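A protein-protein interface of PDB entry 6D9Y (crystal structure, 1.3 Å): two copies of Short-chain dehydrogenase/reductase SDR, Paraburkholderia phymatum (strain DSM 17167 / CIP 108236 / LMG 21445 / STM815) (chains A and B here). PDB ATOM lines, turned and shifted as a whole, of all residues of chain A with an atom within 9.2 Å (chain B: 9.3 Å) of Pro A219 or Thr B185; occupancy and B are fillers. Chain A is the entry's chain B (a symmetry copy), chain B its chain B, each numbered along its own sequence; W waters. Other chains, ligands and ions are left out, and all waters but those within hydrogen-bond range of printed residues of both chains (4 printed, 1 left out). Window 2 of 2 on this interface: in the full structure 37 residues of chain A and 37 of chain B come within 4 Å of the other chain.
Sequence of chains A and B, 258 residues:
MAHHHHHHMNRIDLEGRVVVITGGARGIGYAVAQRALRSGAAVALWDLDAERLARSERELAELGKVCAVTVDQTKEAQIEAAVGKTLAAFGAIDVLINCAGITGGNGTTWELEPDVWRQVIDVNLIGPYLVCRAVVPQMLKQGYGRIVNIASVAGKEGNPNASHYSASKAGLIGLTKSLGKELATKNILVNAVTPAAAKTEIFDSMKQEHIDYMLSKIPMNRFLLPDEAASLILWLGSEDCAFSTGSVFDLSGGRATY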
ATOM      1  N   VAL A 153       4.732  33.146 -14.337  1.00  0.00           N
ATOM      2  CA  VAL A 153       5.124  31.771 -14.628  1.00  0.00           C
ATOM      3  C   VAL A 153       3.898  30.875 -14.777  1.00  0.00           C
ATOM      4  O   VAL A 153       3.936  29.894 -15.539  1.00  0.00           O
ATOM      5  CB  VAL A 153       6.159  31.282 -13.592  1.00  0.00           C
ATOM      6  CG1 VAL A 153       5.532  31.110 -12.247  1.00  0.00           C
ATOM      7  CG2 VAL A 153       6.862  29.973 -14.060  1.00  0.00           C
ATOM      8  N   GLU A 157       2.991  27.666 -17.420  1.00  0.00           N
ATOM      9  CA  GLU A 157       2.953  26.331 -16.841  1.00  0.00           C
ATOM     10  C   GLU A 157       1.572  25.752 -16.593  1.00  0.00           C
ATOM     11  O   GLU A 157       1.453  24.522 -16.544  1.00  0.00           O
ATOM     12  CB  GLU A 157       3.757  26.304 -15.532  1.00  0.00           C
ATOM     13  CG  GLU A 157       5.220  26.681 -15.793  1.00  0.00           C
ATOM     14  CD  GLU A 157       6.188  26.285 -14.713  1.00  0.00           C
ATOM     15  OE1 GLU A 157       7.393  26.535 -14.933  1.00  0.00           O
ATOM     16  OE2 GLU A 157       5.776  25.705 -13.693  1.00  0.00           O
ATOM     17  N   ALA A 196       7.721  34.599 -10.864  1.00  0.00           N
ATOM     18  CA  ALA A 196       7.157  33.718  -9.861  1.00  0.00           C
ATOM     19  C   ALA A 196       6.515  34.587  -8.792  1.00  0.00           C
ATOM     20  O   ALA A 196       6.483  35.817  -8.893  1.00  0.00           O
ATOM     21  CB  ALA A 196       8.249  32.840  -9.245  1.00  0.00           C
ATOM     22  N   MET A 214       3.548  27.330  -4.666  1.00  0.00           N
ATOM     23  CA  MET A 214       4.334  28.206  -5.527  1.00  0.00           C
ATOM     24  C   MET A 214       5.786  28.304  -5.048  1.00  0.00           C
ATOM     25  O   MET A 214       6.714  28.238  -5.864  1.00  0.00           O
ATOM     26  CB  MET A 214       3.672  29.586  -5.636  1.00  0.00           C
ATOM     27  CG  MET A 214       2.300  29.575  -6.331  1.00  0.00           C
ATOM     28  SD  MET A 214       1.704  31.252  -6.728  1.00  0.00           S
ATOM     29  CE  MET A 214       1.440  31.915  -5.094  1.00  0.00           C
ATOM     30  N   LEU A 215       5.997  28.402  -3.724  1.00  0.00           N
ATOM     31  CA  LEU A 215       7.357  28.524  -3.200  1.00  0.00           C
ATOM     32  C   LEU A 215       8.167  27.254  -3.435  1.00  0.00           C
ATOM     33  O   LEU A 215       9.356  27.331  -3.773  1.00  0.00           O
ATOM     34  CB  LEU A 215       7.346  28.883  -1.708  1.00  0.00           C
ATOM     35  CG  LEU A 215       8.727  29.001  -1.022  1.00  0.00           C
ATOM     36  CD1 LEU A 215       9.600  30.137  -1.611  1.00  0.00           C
ATOM     37  CD2 LEU A 215       8.593  29.154   0.492  1.00  0.00           C
ATOM     38  N   SER A 216       7.555  26.081  -3.253  1.00  0.00           N
ATOM     39  CA  SER A 216       8.284  24.817  -3.345  1.00  0.00           C
ATOM     40  C   SER A 216       8.887  24.589  -4.729  1.00  0.00           C
ATOM     41  O   SER A 216       9.803  23.770  -4.878  1.00  0.00           O
ATOM     42  CB  SER A 216       7.319  23.673  -3.029  1.00  0.00           C
ATOM     43  OG  SER A 216       6.309  23.571  -4.025  1.00  0.00           O
ATOM     44  N   LYS A 217       8.376  25.259  -5.737  1.00  0.00           N
ATOM     45  CA  LYS A 217       8.821  25.024  -7.093  1.00  0.00           C
ATOM     46  C   LYS A 217       9.976  25.931  -7.509  1.00  0.00           C
ATOM     47  O   LYS A 217      10.377  25.890  -8.668  1.00  0.00           O
ATOM     48  CB  LYS A 217       7.627  25.159  -8.033  1.00  0.00           C
ATOM     49  CG  LYS A 217       6.659  23.973  -7.861  1.00  0.00           C
ATOM     50  CD  LYS A 217       5.353  24.157  -8.604  1.00  0.00           C
ATOM     51  CE  LYS A 217       5.532  24.031 -10.106  1.00  0.00           C
ATOM     52  NZ  LYS A 217       5.763  22.636 -10.571  1.00  0.00           N
ATOM     53  N   ILE A 218      10.511  26.748  -6.597  1.00  0.00           N
ATOM     54  CA  ILE A 218      11.510  27.770  -6.909  1.00  0.00           C
ATOM     55  C   ILE A 218      12.894  27.271  -6.484  1.00  0.00           C
ATOM     56  O   ILE A 218      13.186  27.233  -5.272  1.00  0.00           O
ATOM     57  CB  ILE A 218      11.181  29.105  -6.232  1.00  0.00           C
ATOM     58  CG1 ILE A 218       9.788  29.590  -6.673  1.00  0.00           C
ATOM     59  CG2 ILE A 218      12.253  30.153  -6.599  1.00  0.00           C
ATOM     60  CD1 ILE A 218       9.326  30.854  -5.955  1.00  0.00           C
ATOM     61  N   PRO A 219      13.792  26.954  -7.425  1.00  0.00           N
ATOM     62  CA  PRO A 219      15.150  26.509  -7.045  1.00  0.00           C
ATOM     63  C   PRO A 219      15.929  27.500  -6.195  1.00  0.00           C
ATOM     64  O   PRO A 219      16.728  27.090  -5.345  1.00  0.00           O
ATOM     65  CB  PRO A 219      15.823  26.260  -8.410  1.00  0.00           C
ATOM     66  CG  PRO A 219      14.685  25.836  -9.303  1.00  0.00           C
ATOM     67  CD  PRO A 219      13.541  26.764  -8.871  1.00  0.00           C
ATOM     68  N   MET A 220      15.735  28.807  -6.400  1.00  0.00           N
ATOM     69  CA  MET A 220      16.399  29.810  -5.565  1.00  0.00           C
ATOM     70  C   MET A 220      15.877  29.833  -4.134  1.00  0.00           C
ATOM     71  O   MET A 220      16.468  30.529  -3.295  1.00  0.00           O
ATOM     72  CB  MET A 220      16.356  31.188  -6.218  1.00  0.00           C
ATOM     73  CG  MET A 220      17.295  31.246  -7.426  1.00  0.00           C
ATOM     74  SD  MET A 220      17.411  32.836  -8.238  1.00  0.00           S
ATOM     75  CE  MET A 220      18.334  33.760  -7.010  1.00  0.00           C
ATOM     76  N   ASN A 221      14.776  29.139  -3.837  1.00  0.00           N
ATOM     77  CA  ASN A 221      14.347  28.908  -2.460  1.00  0.00           C
ATOM     78  C   ASN A 221      13.919  30.186  -1.727  1.00  0.00           C
ATOM     79  O   ASN A 221      14.077  30.277  -0.507  1.00  0.00           O
ATOM     80  CB  ASN A 221      15.421  28.146  -1.671  1.00  0.00           C
ATOM     81  CG  ASN A 221      14.865  27.434  -0.484  1.00  0.00           C
ATOM     82  OD1 ASN A 221      13.734  26.971  -0.510  1.00  0.00           O
ATOM     83  ND2 ASN A 221      15.653  27.356   0.580  1.00  0.00           N
ATOM     84  N   ARG A 222      13.374  31.158  -2.447  1.00  0.00           N
ATOM     85  CA  ARG A 222      12.835  32.374  -1.856  1.00  0.00           C
ATOM     86  C   ARG A 222      11.897  32.982  -2.886  1.00  0.00           C
ATOM     87  O   ARG A 222      11.881  32.587  -4.054  1.00  0.00           O
ATOM     88  CB  ARG A 222      13.938  33.383  -1.506  1.00  0.00           C
ATOM     89  CG  ARG A 222      14.673  33.925  -2.751  1.00  0.00           C
ATOM     90  CD  ARG A 222      15.628  35.015  -2.339  1.00  0.00           C
ATOM     91  NE  ARG A 222      16.487  35.553  -3.402  1.00  0.00           N
ATOM     92  CZ  ARG A 222      16.165  36.560  -4.220  1.00  0.00           C
ATOM     93  NH1 ARG A 222      14.957  37.113  -4.203  1.00  0.00           N
ATOM     94  NH2 ARG A 222      17.081  37.002  -5.073  1.00  0.00           N
ATOM     95  N   PHE A 223      11.126  33.968  -2.446  1.00  0.00           N
ATOM     96  CA  PHE A 223      10.253  34.689  -3.360  1.00  0.00           C
ATOM     97  C   PHE A 223      10.991  35.813  -4.100  1.00  0.00           C
ATOM     98  O   PHE A 223      12.022  36.323  -3.663  1.00  0.00           O
ATOM     99  CB  PHE A 223       9.070  35.281  -2.605  1.00  0.00           C
ATOM    100  CG  PHE A 223       8.114  34.251  -2.074  1.00  0.00           C
ATOM    101  CD1 PHE A 223       7.405  33.440  -2.939  1.00  0.00           C
ATOM    102  CD2 PHE A 223       7.907  34.112  -0.707  1.00  0.00           C
ATOM    103  CE1 PHE A 223       6.504  32.495  -2.451  1.00  0.00           C
ATOM    104  CE2 PHE A 223       7.011  33.172  -0.216  1.00  0.00           C
ATOM    105  CZ  PHE A 223       6.310  32.367  -1.096  1.00  0.00           C
ATOM    106  N   ASP A 250      12.171  35.790 -18.296  1.00  0.00           N
ATOM    107  CA  ASP A 250      11.763  35.050 -17.104  1.00  0.00           C
ATOM    108  C   ASP A 250      12.233  35.681 -15.796  1.00  0.00           C
ATOM    109  O   ASP A 250      13.379  36.139 -15.697  1.00  0.00           O
ATOM    110  CB  ASP A 250      12.267  33.608 -17.175  1.00  0.00           C
ATOM    111  CG  ASP A 250      11.589  32.747 -16.158  1.00  0.00           C
ATOM    112  OD1 ASP A 250      10.381  32.433 -16.332  1.00  0.00           O
ATOM    113  OD2 ASP A 250      12.243  32.442 -15.130  1.00  0.00           O
ATOM    114  N   SER A 252      11.463  33.752 -12.640  1.00  0.00           N
ATOM    115  CA  SER A 252      10.912  32.663 -11.841  1.00  0.00           C
ATOM    116  C   SER A 252      11.921  32.019 -10.893  1.00  0.00           C
ATOM    117  O   SER A 252      11.624  30.975 -10.310  1.00  0.00           O
ATOM    118  CB  SER A 252      10.246  31.612 -12.744  1.00  0.00           C
ATOM    119  OG  SER A 252      11.202  30.784 -13.394  1.00  0.00           O
ATOM    120  N   GLY A 253      13.124  32.586 -10.758  1.00  0.00           N
ATOM    121  CA  GLY A 253      14.060  32.054  -9.767  1.00  0.00           C
ATOM    122  C   GLY A 253      14.545  30.658 -10.088  1.00  0.00           C
ATOM    123  O   GLY A 253      14.823  29.870  -9.167  1.00  0.00           O
ATOM    124  N   GLY A 254      14.638  30.323 -11.377  1.00  0.00           N
ATOM    125  CA  GLY A 254      15.091  29.017 -11.811  1.00  0.00           C
ATOM    126  C   GLY A 254      13.990  28.025 -12.096  1.00  0.00           C
ATOM    127  O   GLY A 254      14.285  26.917 -12.539  1.00  0.00           O
ATOM    128  N   ARG A 255      12.731  28.360 -11.793  1.00  0.00           N
ATOM    129  CA  ARG A 255      11.653  27.388 -11.935  1.00  0.00           C
ATOM    130  C   ARG A 255      11.380  27.033 -13.396  1.00  0.00           C
ATOM    131  O   ARG A 255      11.278  25.844 -13.759  1.00  0.00           O
ATOM    132  CB  ARG A 255      10.398  27.941 -11.261  1.00  0.00           C
ATOM    133  CG  ARG A 255       9.146  27.128 -11.589  1.00  0.00           C
ATOM    134  CD  ARG A 255       7.974  27.585 -10.756  1.00  0.00           C
ATOM    135  NE  ARG A 255       6.728  27.048 -11.313  1.00  0.00           N
ATOM    136  CZ  ARG A 255       5.515  27.418 -10.917  1.00  0.00           C
ATOM    137  NH1 ARG A 255       5.353  28.252  -9.882  1.00  0.00           N
ATOM    138  NH2 ARG A 255       4.455  26.938 -11.550  1.00  0.00           N
ATOM    139  N   ALA A 256      11.161  28.047 -14.236  1.00  0.00           N
ATOM    140  CA  ALA A 256      10.647  27.785 -15.582  1.00  0.00           C
ATOM    141  C   ALA A 256      11.655  26.979 -16.399  1.00  0.00           C
ATOM    142  O   ALA A 256      12.868  27.169 -16.287  1.00  0.00           O
ATOM    143  CB  ALA A 256      10.335  29.104 -16.313  1.00  0.00           C
ATOM    144  N   THR A 257      11.147  26.107 -17.258  1.00  0.00           N
ATOM    145  CA  THR A 257      11.988  25.252 -18.108  1.00  0.00           C
ATOM    146  C   THR A 257      11.998  25.705 -19.555  1.00  0.00           C
ATOM    147  O   THR A 257      12.591  25.014 -20.402  1.00  0.00           O
ATOM    148  CB  THR A 257      11.618  23.782 -17.962  1.00  0.00           C
ATOM    149  OG1 THR A 257      10.218  23.617 -18.275  1.00  0.00           O
ATOM    150  CG2 THR A 257      11.903  23.311 -16.543  1.00  0.00           C
ATOM    151  N   LEU B 140      32.413  29.663  -6.742  1.00  0.00           N
ATOM    152  CA  LEU B 140      32.027  29.187  -5.415  1.00  0.00           C
ATOM    153  C   LEU B 140      32.965  29.730  -4.347  1.00  0.00           C
ATOM    154  O   LEU B 140      32.511  30.142  -3.269  1.00  0.00           O
ATOM    155  CB  LEU B 140      32.009  27.661  -5.391  1.00  0.00           C
ATOM    156  CG  LEU B 140      30.855  27.007  -6.151  1.00  0.00           C
ATOM    157  CD1 LEU B 140      31.132  25.530  -6.363  1.00  0.00           C
ATOM    158  CD2 LEU B 140      29.514  27.216  -5.453  1.00  0.00           C
ATOM    159  N   GLY B 143      31.915  33.196  -3.558  1.00  0.00           N
ATOM    160  CA  GLY B 143      30.536  33.446  -3.186  1.00  0.00           C
ATOM    161  C   GLY B 143      29.786  34.326  -4.163  1.00  0.00           C
ATOM    162  O   GLY B 143      28.832  35.011  -3.754  1.00  0.00           O
ATOM    163  N   TYR B 144      30.174  34.337  -5.448  1.00  0.00           N
ATOM    164  CA  TYR B 144      29.530  35.187  -6.449  1.00  0.00           C
ATOM    165  C   TYR B 144      29.949  34.751  -7.837  1.00  0.00           C
ATOM    166  O   TYR B 144      31.139  34.534  -8.084  1.00  0.00           O
ATOM    167  CB  TYR B 144      29.934  36.667  -6.286  1.00  0.00           C
ATOM    168  CG  TYR B 144      29.240  37.548  -7.309  1.00  0.00           C
ATOM    169  CD1 TYR B 144      27.930  37.964  -7.107  1.00  0.00           C
ATOM    170  CD2 TYR B 144      29.865  37.908  -8.513  1.00  0.00           C
ATOM    171  CE1 TYR B 144      27.253  38.714  -8.059  1.00  0.00           C
ATOM    172  CE2 TYR B 144      29.197  38.686  -9.461  1.00  0.00           C
ATOM    173  CZ  TYR B 144      27.891  39.082  -9.233  1.00  0.00           C
ATOM    174  OH  TYR B 144      27.199  39.842 -10.162  1.00  0.00           O
ATOM    175  N   LYS B 177      20.369  25.130 -18.339  1.00  0.00           N
ATOM    176  CA  LYS B 177      19.257  24.852 -17.434  1.00  0.00           C
ATOM    177  C   LYS B 177      19.693  23.985 -16.255  1.00  0.00           C
ATOM    178  O   LYS B 177      19.312  24.253 -15.104  1.00  0.00           O
ATOM    179  CB  LYS B 177      18.130  24.192 -18.236  1.00  0.00           C
ATOM    180  CG  LYS B 177      17.456  25.149 -19.237  1.00  0.00           C
ATOM    181  CD  LYS B 177      16.395  24.432 -20.057  1.00  0.00           C
ATOM    182  CE  LYS B 177      15.743  25.390 -21.066  1.00  0.00           C
ATOM    183  NZ  LYS B 177      14.814  24.625 -21.966  1.00  0.00           N
ATOM    184  N   SER B 178      20.484  22.932 -16.518  1.00  0.00           N
ATOM    185  CA  SER B 178      20.973  22.068 -15.431  1.00  0.00           C
ATOM    186  C   SER B 178      21.889  22.837 -14.485  1.00  0.00           C
ATOM    187  O   SER B 178      21.720  22.785 -13.247  1.00  0.00           O
ATOM    188  CB  SER B 178      21.747  20.869 -16.009  1.00  0.00           C
ATOM    189  OG  SER B 178      20.906  19.901 -16.620  1.00  0.00           O
ATOM    190  N   LEU B 179      22.873  23.550 -15.052  1.00  0.00           N
ATOM    191  CA  LEU B 179      23.876  24.230 -14.239  1.00  0.00           C
ATOM    192  C   LEU B 179      23.237  25.334 -13.410  1.00  0.00           C
ATOM    193  O   LEU B 179      23.567  25.509 -12.222  1.00  0.00           O
ATOM    194  CB  LEU B 179      24.979  24.773 -15.160  1.00  0.00           C
ATOM    195  CG  LEU B 179      26.144  25.471 -14.453  1.00  0.00           C
ATOM    196  CD1 LEU B 179      26.801  24.562 -13.442  1.00  0.00           C
ATOM    197  CD2 LEU B 179      27.178  25.927 -15.481  1.00  0.00           C
ATOM    198  N   GLY B 180      22.276  26.068 -13.982  1.00  0.00           N
ATOM    199  CA  GLY B 180      21.615  27.112 -13.212  1.00  0.00           C
ATOM    200  C   GLY B 180      20.888  26.549 -12.011  1.00  0.00           C
ATOM    201  O   GLY B 180      20.978  27.086 -10.904  1.00  0.00           O
ATOM    202  N   LYS B 181      20.195  25.417 -12.188  1.00  0.00           N
ATOM    203  CA  LYS B 181      19.512  24.826 -11.038  1.00  0.00           C
ATOM    204  C   LYS B 181      20.485  24.252 -10.013  1.00  0.00           C
ATOM    205  O   LYS B 181      20.232  24.348  -8.804  1.00  0.00           O
ATOM    206  CB  LYS B 181      18.446  23.830 -11.491  1.00  0.00           C
ATOM    207  CG  LYS B 181      17.229  24.583 -12.098  1.00  0.00           C
ATOM    208  CD  LYS B 181      15.995  23.710 -12.334  1.00  0.00           C
ATOM    209  CE  LYS B 181      16.140  22.755 -13.482  1.00  0.00           C
ATOM    210  NZ  LYS B 181      16.438  23.437 -14.801  1.00  0.00           N
ATOM    211  N   GLU B 182      21.642  23.743 -10.442  1.00  0.00           N
ATOM    212  CA  GLU B 182      22.642  23.248  -9.490  1.00  0.00           C
ATOM    213  C   GLU B 182      23.198  24.371  -8.633  1.00  0.00           C
ATOM    214  O   GLU B 182      23.600  24.124  -7.487  1.00  0.00           O
ATOM    215  CB  GLU B 182      23.797  22.577 -10.240  1.00  0.00           C
ATOM    216  CG  GLU B 182      23.393  21.261 -10.900  1.00  0.00           C
ATOM    217  CD  GLU B 182      24.417  20.733 -11.884  1.00  0.00           C
ATOM    218  OE1 GLU B 182      25.494  21.334 -12.087  1.00  0.00           O
ATOM    219  OE2 GLU B 182      24.093  19.673 -12.494  1.00  0.00           O
ATOM    220  N   LEU B 183      23.220  25.601  -9.138  1.00  0.00           N
ATOM    221  CA  LEU B 183      23.858  26.719  -8.446  1.00  0.00           C
ATOM    222  C   LEU B 183      22.859  27.722  -7.891  1.00  0.00           C
ATOM    223  O   LEU B 183      23.271  28.764  -7.381  1.00  0.00           O
ATOM    224  CB  LEU B 183      24.823  27.405  -9.412  1.00  0.00           C
ATOM    225  CG  LEU B 183      26.050  26.560  -9.739  1.00  0.00           C
ATOM    226  CD1 LEU B 183      26.842  27.242 -10.864  1.00  0.00           C
ATOM    227  CD2 LEU B 183      26.952  26.399  -8.516  1.00  0.00           C
ATOM    228  N   ALA B 184      21.558  27.399  -7.905  1.00  0.00           N
ATOM    229  CA  ALA B 184      20.526  28.391  -7.601  1.00  0.00           C
ATOM    230  C   ALA B 184      20.590  28.929  -6.176  1.00  0.00           C
ATOM    231  O   ALA B 184      20.102  30.039  -5.928  1.00  0.00           O
ATOM    232  CB  ALA B 184      19.145  27.780  -7.853  1.00  0.00           C
ATOM    233  N   THR B 185      21.140  28.158  -5.231  1.00  0.00           N
ATOM    234  CA  THR B 185      21.273  28.611  -3.846  1.00  0.00           C
ATOM    235  C   THR B 185      22.692  29.069  -3.528  1.00  0.00           C
ATOM    236  O   THR B 185      22.995  29.375  -2.361  1.00  0.00           O
ATOM    237  CB  THR B 185      20.836  27.535  -2.835  1.00  0.00           C
ATOM    238  OG1 THR B 185      21.746  26.449  -2.868  1.00  0.00           O
ATOM    239  CG2 THR B 185      19.404  27.049  -3.145  1.00  0.00           C
ATOM    240  N   LYS B 186      23.557  29.196  -4.536  1.00  0.00           N
ATOM    241  CA  LYS B 186      24.976  29.465  -4.327  1.00  0.00           C
ATOM    242  C   LYS B 186      25.399  30.828  -4.853  1.00  0.00           C
ATOM    243  O   LYS B 186      26.596  31.099  -4.944  1.00  0.00           O
ATOM    244  CB  LYS B 186      25.854  28.378  -4.950  1.00  0.00           C
ATOM    245  CG  LYS B 186      25.623  26.974  -4.405  1.00  0.00           C
ATOM    246  CD  LYS B 186      25.731  26.893  -2.886  1.00  0.00           C
ATOM    247  CE  LYS B 186      27.137  27.195  -2.359  1.00  0.00           C
ATOM    248  NZ  LYS B 186      27.307  26.735  -0.934  1.00  0.00           N
ATOM    249  N   ASN B 187      24.457  31.698  -5.204  1.00  0.00           N
ATOM    250  CA  ASN B 187      24.767  33.077  -5.593  1.00  0.00           C
ATOM    251  C   ASN B 187      25.510  33.170  -6.927  1.00  0.00           C
ATOM    252  O   ASN B 187      26.218  34.160  -7.174  1.00  0.00           O
ATOM    253  CB  ASN B 187      25.503  33.846  -4.480  1.00  0.00           C
ATOM    254  CG  ASN B 187      25.242  35.340  -4.523  1.00  0.00           C
ATOM    255  OD1 ASN B 187      24.136  35.768  -4.848  1.00  0.00           O
ATOM    256  ND2 ASN B 187      26.240  36.135  -4.198  1.00  0.00           N
ATOM    257  N   ILE B 188      25.346  32.163  -7.793  1.00  0.00           N
ATOM    258  CA  ILE B 188      25.958  32.136  -9.126  1.00  0.00           C
ATOM    259  C   ILE B 188      24.811  31.860 -10.083  1.00  0.00           C
ATOM    260  O   ILE B 188      24.240  30.767 -10.052  1.00  0.00           O
ATOM    261  CB  ILE B 188      27.018  31.031  -9.226  1.00  0.00           C
ATOM    262  CG1 ILE B 188      28.155  31.259  -8.208  1.00  0.00           C
ATOM    263  CG2 ILE B 188      27.567  30.953 -10.664  1.00  0.00           C
ATOM    264  CD1 ILE B 188      28.919  29.984  -7.883  1.00  0.00           C
ATOM    265  N   LEU B 189      24.417  32.862 -10.887  1.00  0.00           N
ATOM    266  CA  LEU B 189      23.293  32.719 -11.804  1.00  0.00           C
ATOM    267  C   LEU B 189      23.829  32.464 -13.210  1.00  0.00           C
ATOM    268  O   LEU B 189      24.896  32.972 -13.589  1.00  0.00           O
ATOM    269  CB  LEU B 189      22.370  33.947 -11.767  1.00  0.00           C
ATOM    270  CG  LEU B 189      21.940  34.346 -10.347  1.00  0.00           C
ATOM    271  CD1 LEU B 189      20.928  35.489 -10.443  1.00  0.00           C
ATOM    272  CD2 LEU B 189      21.375  33.169  -9.533  1.00  0.00           C
ATOM    273  N   PHE B 243      17.093  37.230 -10.242  1.00  0.00           N
ATOM    274  CA  PHE B 243      16.071  36.212  -9.987  1.00  0.00           C
ATOM    275  C   PHE B 243      15.737  35.482 -11.280  1.00  0.00           C
ATOM    276  O   PHE B 243      14.602  35.034 -11.480  1.00  0.00           O
ATOM    277  CB  PHE B 243      14.828  36.805  -9.292  1.00  0.00           C
ATOM    278  CG  PHE B 243      14.061  35.807  -8.453  1.00  0.00           C
ATOM    279  CD1 PHE B 243      14.609  35.309  -7.270  1.00  0.00           C
ATOM    280  CD2 PHE B 243      12.790  35.364  -8.832  1.00  0.00           C
ATOM    281  CE1 PHE B 243      13.914  34.393  -6.501  1.00  0.00           C
ATOM    282  CE2 PHE B 243      12.092  34.454  -8.042  1.00  0.00           C
ATOM    283  CZ  PHE B 243      12.647  33.986  -6.882  1.00  0.00           C
ATOM    284  N   SER B 244      16.731  35.371 -12.153  1.00  0.00           N
ATOM    285  CA  SER B 244      16.621  34.667 -13.426  1.00  0.00           C
ATOM    286  C   SER B 244      17.821  33.747 -13.494  1.00  0.00           C
ATOM    287  O   SER B 244      18.968  34.222 -13.434  1.00  0.00           O
ATOM    288  CB  SER B 244      16.679  35.646 -14.610  1.00  0.00           C
ATOM    289  OG  SER B 244      15.751  36.700 -14.458  1.00  0.00           O
ATOM    290  N   THR B 245      17.573  32.436 -13.579  1.00  0.00           N
ATOM    291  CA  THR B 245      18.665  31.486 -13.703  1.00  0.00           C
ATOM    292  C   THR B 245      18.164  30.234 -14.402  1.00  0.00           C
ATOM    293  O   THR B 245      16.973  29.913 -14.353  1.00  0.00           O
ATOM    294  CB  THR B 245      19.342  31.202 -12.349  1.00  0.00           C
ATOM    295  OG1 THR B 245      20.610  30.612 -12.611  1.00  0.00           O
ATOM    296  CG2 THR B 245      18.492  30.305 -11.457  1.00  0.00           C
ATOM    297  N   GLY B 246      19.081  29.537 -15.067  1.00  0.00           N
ATOM    298  CA  GLY B 246      18.688  28.464 -15.970  1.00  0.00           C
ATOM    299  C   GLY B 246      17.740  28.904 -17.060  1.00  0.00           C
ATOM    300  O   GLY B 246      16.931  28.080 -17.517  1.00  0.00           O
HETATM  301  O   HOH W   1      14.474  27.688 -18.711  1.00  0.00           O
HETATM  302  O   HOH W   2      14.661  31.783 -13.935  1.00  0.00           O
HETATM  303  O   HOH W   3      15.052  25.796 -14.935  1.00  0.00           O
HETATM  304  O   HOH W   4      14.408  29.323 -15.403  1.00  0.00           O
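The side-chain amino group (NZ) of Lys B177 lies within hydrogen-bond range of the backbone carbonyl oxygen (O) of Thr A257 (2.7 Å).
O of Phe B243 sits at hydrogen-bond distance from N of Gly A253 (2.9 Å).
OG of Ser B244 sits at hydrogen-bond distance from O of Asp A250.
O of Lys B177 sits at hydrogen-bond distance from NZ of Lys B181 (3.0 Å).
The backbone NH (N) of Met A220 sits at hydrogen-bond distance from the backbone carbonyl oxygen (O) of Gly A253, at 3.1 Å.
OD2 of Asp A250 sits at hydrogen-bond distance from OG of Ser A252.
N of Arg A255 lies within hydrogen-bond range of OG of Ser A252 (3.3 Å).
The side-chain hydroxyl of Ser A252 is in hydrogen-bond range of the backbone NH of Ala A256 (2.9 Å).
Ile A218 touches Phe B243 (CG2 to CZ, 3.9 Å).
Pro A219 touches Ala B184.
O of Pro A219 touches CG2 of Thr B185, 3.5 Å away.
CG of Met A220 touches O of Ala B184, at 3.4 Å.
CD2 of Leu B189 touches CE of Met A220, 3.995 Å away.
SD of Met A220 touches CD1 of Phe B243, 3.9 Å away.
Phe B243 touches Phe A223.
O of Phe B243 touches N of Ser A252 (3.6 Å).
Gly A254 touches Lys B181.
CA of Gly A254 touches O of Thr B245 (3.3 Å).
Of chain B, only Lys B181 (3.9 Å), Ala B184 (3.6 Å) and Thr B185 (3.5 Å) come within 4 Å of Pro A219.
Asn A221 touches none of the printed residues of chain B.
Gly A254 touches just these residues of chain B: Lys B181 (3.6 Å) and Thr B245 (3.3 Å).
Ala A256 touches none of the printed residues of chain B.
Of the printed residues of chain B, Thr A257 touches Lys B177.
Printed residues of chain A within 4 Å of Lys B181: Pro A219 (3.9 Å) and Gly A254 (3.6 Å).
Printed residues of chain A within 4 Å of Thr B185: Pro A219 (3.5 Å).
Of the printed residues of chain A, Ser B244 touches Asp A250.
The nearest printed residue of chain A that does not touch Thr B185 is Asn A221 (4.4 Å).
The nearest printed residue of chain A that does not touch Ser B244 is Met A220 (4.7 Å).
Of the 20 printed residues of chain A, 10 touch a printed residue of chain B.
Hydrophobic or aromatic side chains of chain A that line the printed part of chain B: Ile A218, Pro A219 and Met A220.
Of the 20 printed residues of chain B, 8 touch a printed residue of chain A.
Among the printed residues, 15 pairs touch across the chains.
No position is printed for both chains.
Of the 15 pairs that touch across the chains among the printed residues, none has its exchanged pair printed and touching as well.
Water W1 bridges the backbone carbonyl oxygen (O) of Gly B246 (2.8 Å) and the backbone carbonyl oxygen (O) of Ala A256 (3.0 Å).
Water W2 lies within hydrogen-bond range of OD2 of Asp A250 (2.8 Å), N of Gly A254 (2.9 Å) and O of Thr B245 (3.0 Å).
Water W4 bridges the backbone carbonyl oxygen (O) of Ala A256 (2.8 Å) and the backbone carbonyl oxygen (O) of Thr B245 (2.8 Å).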
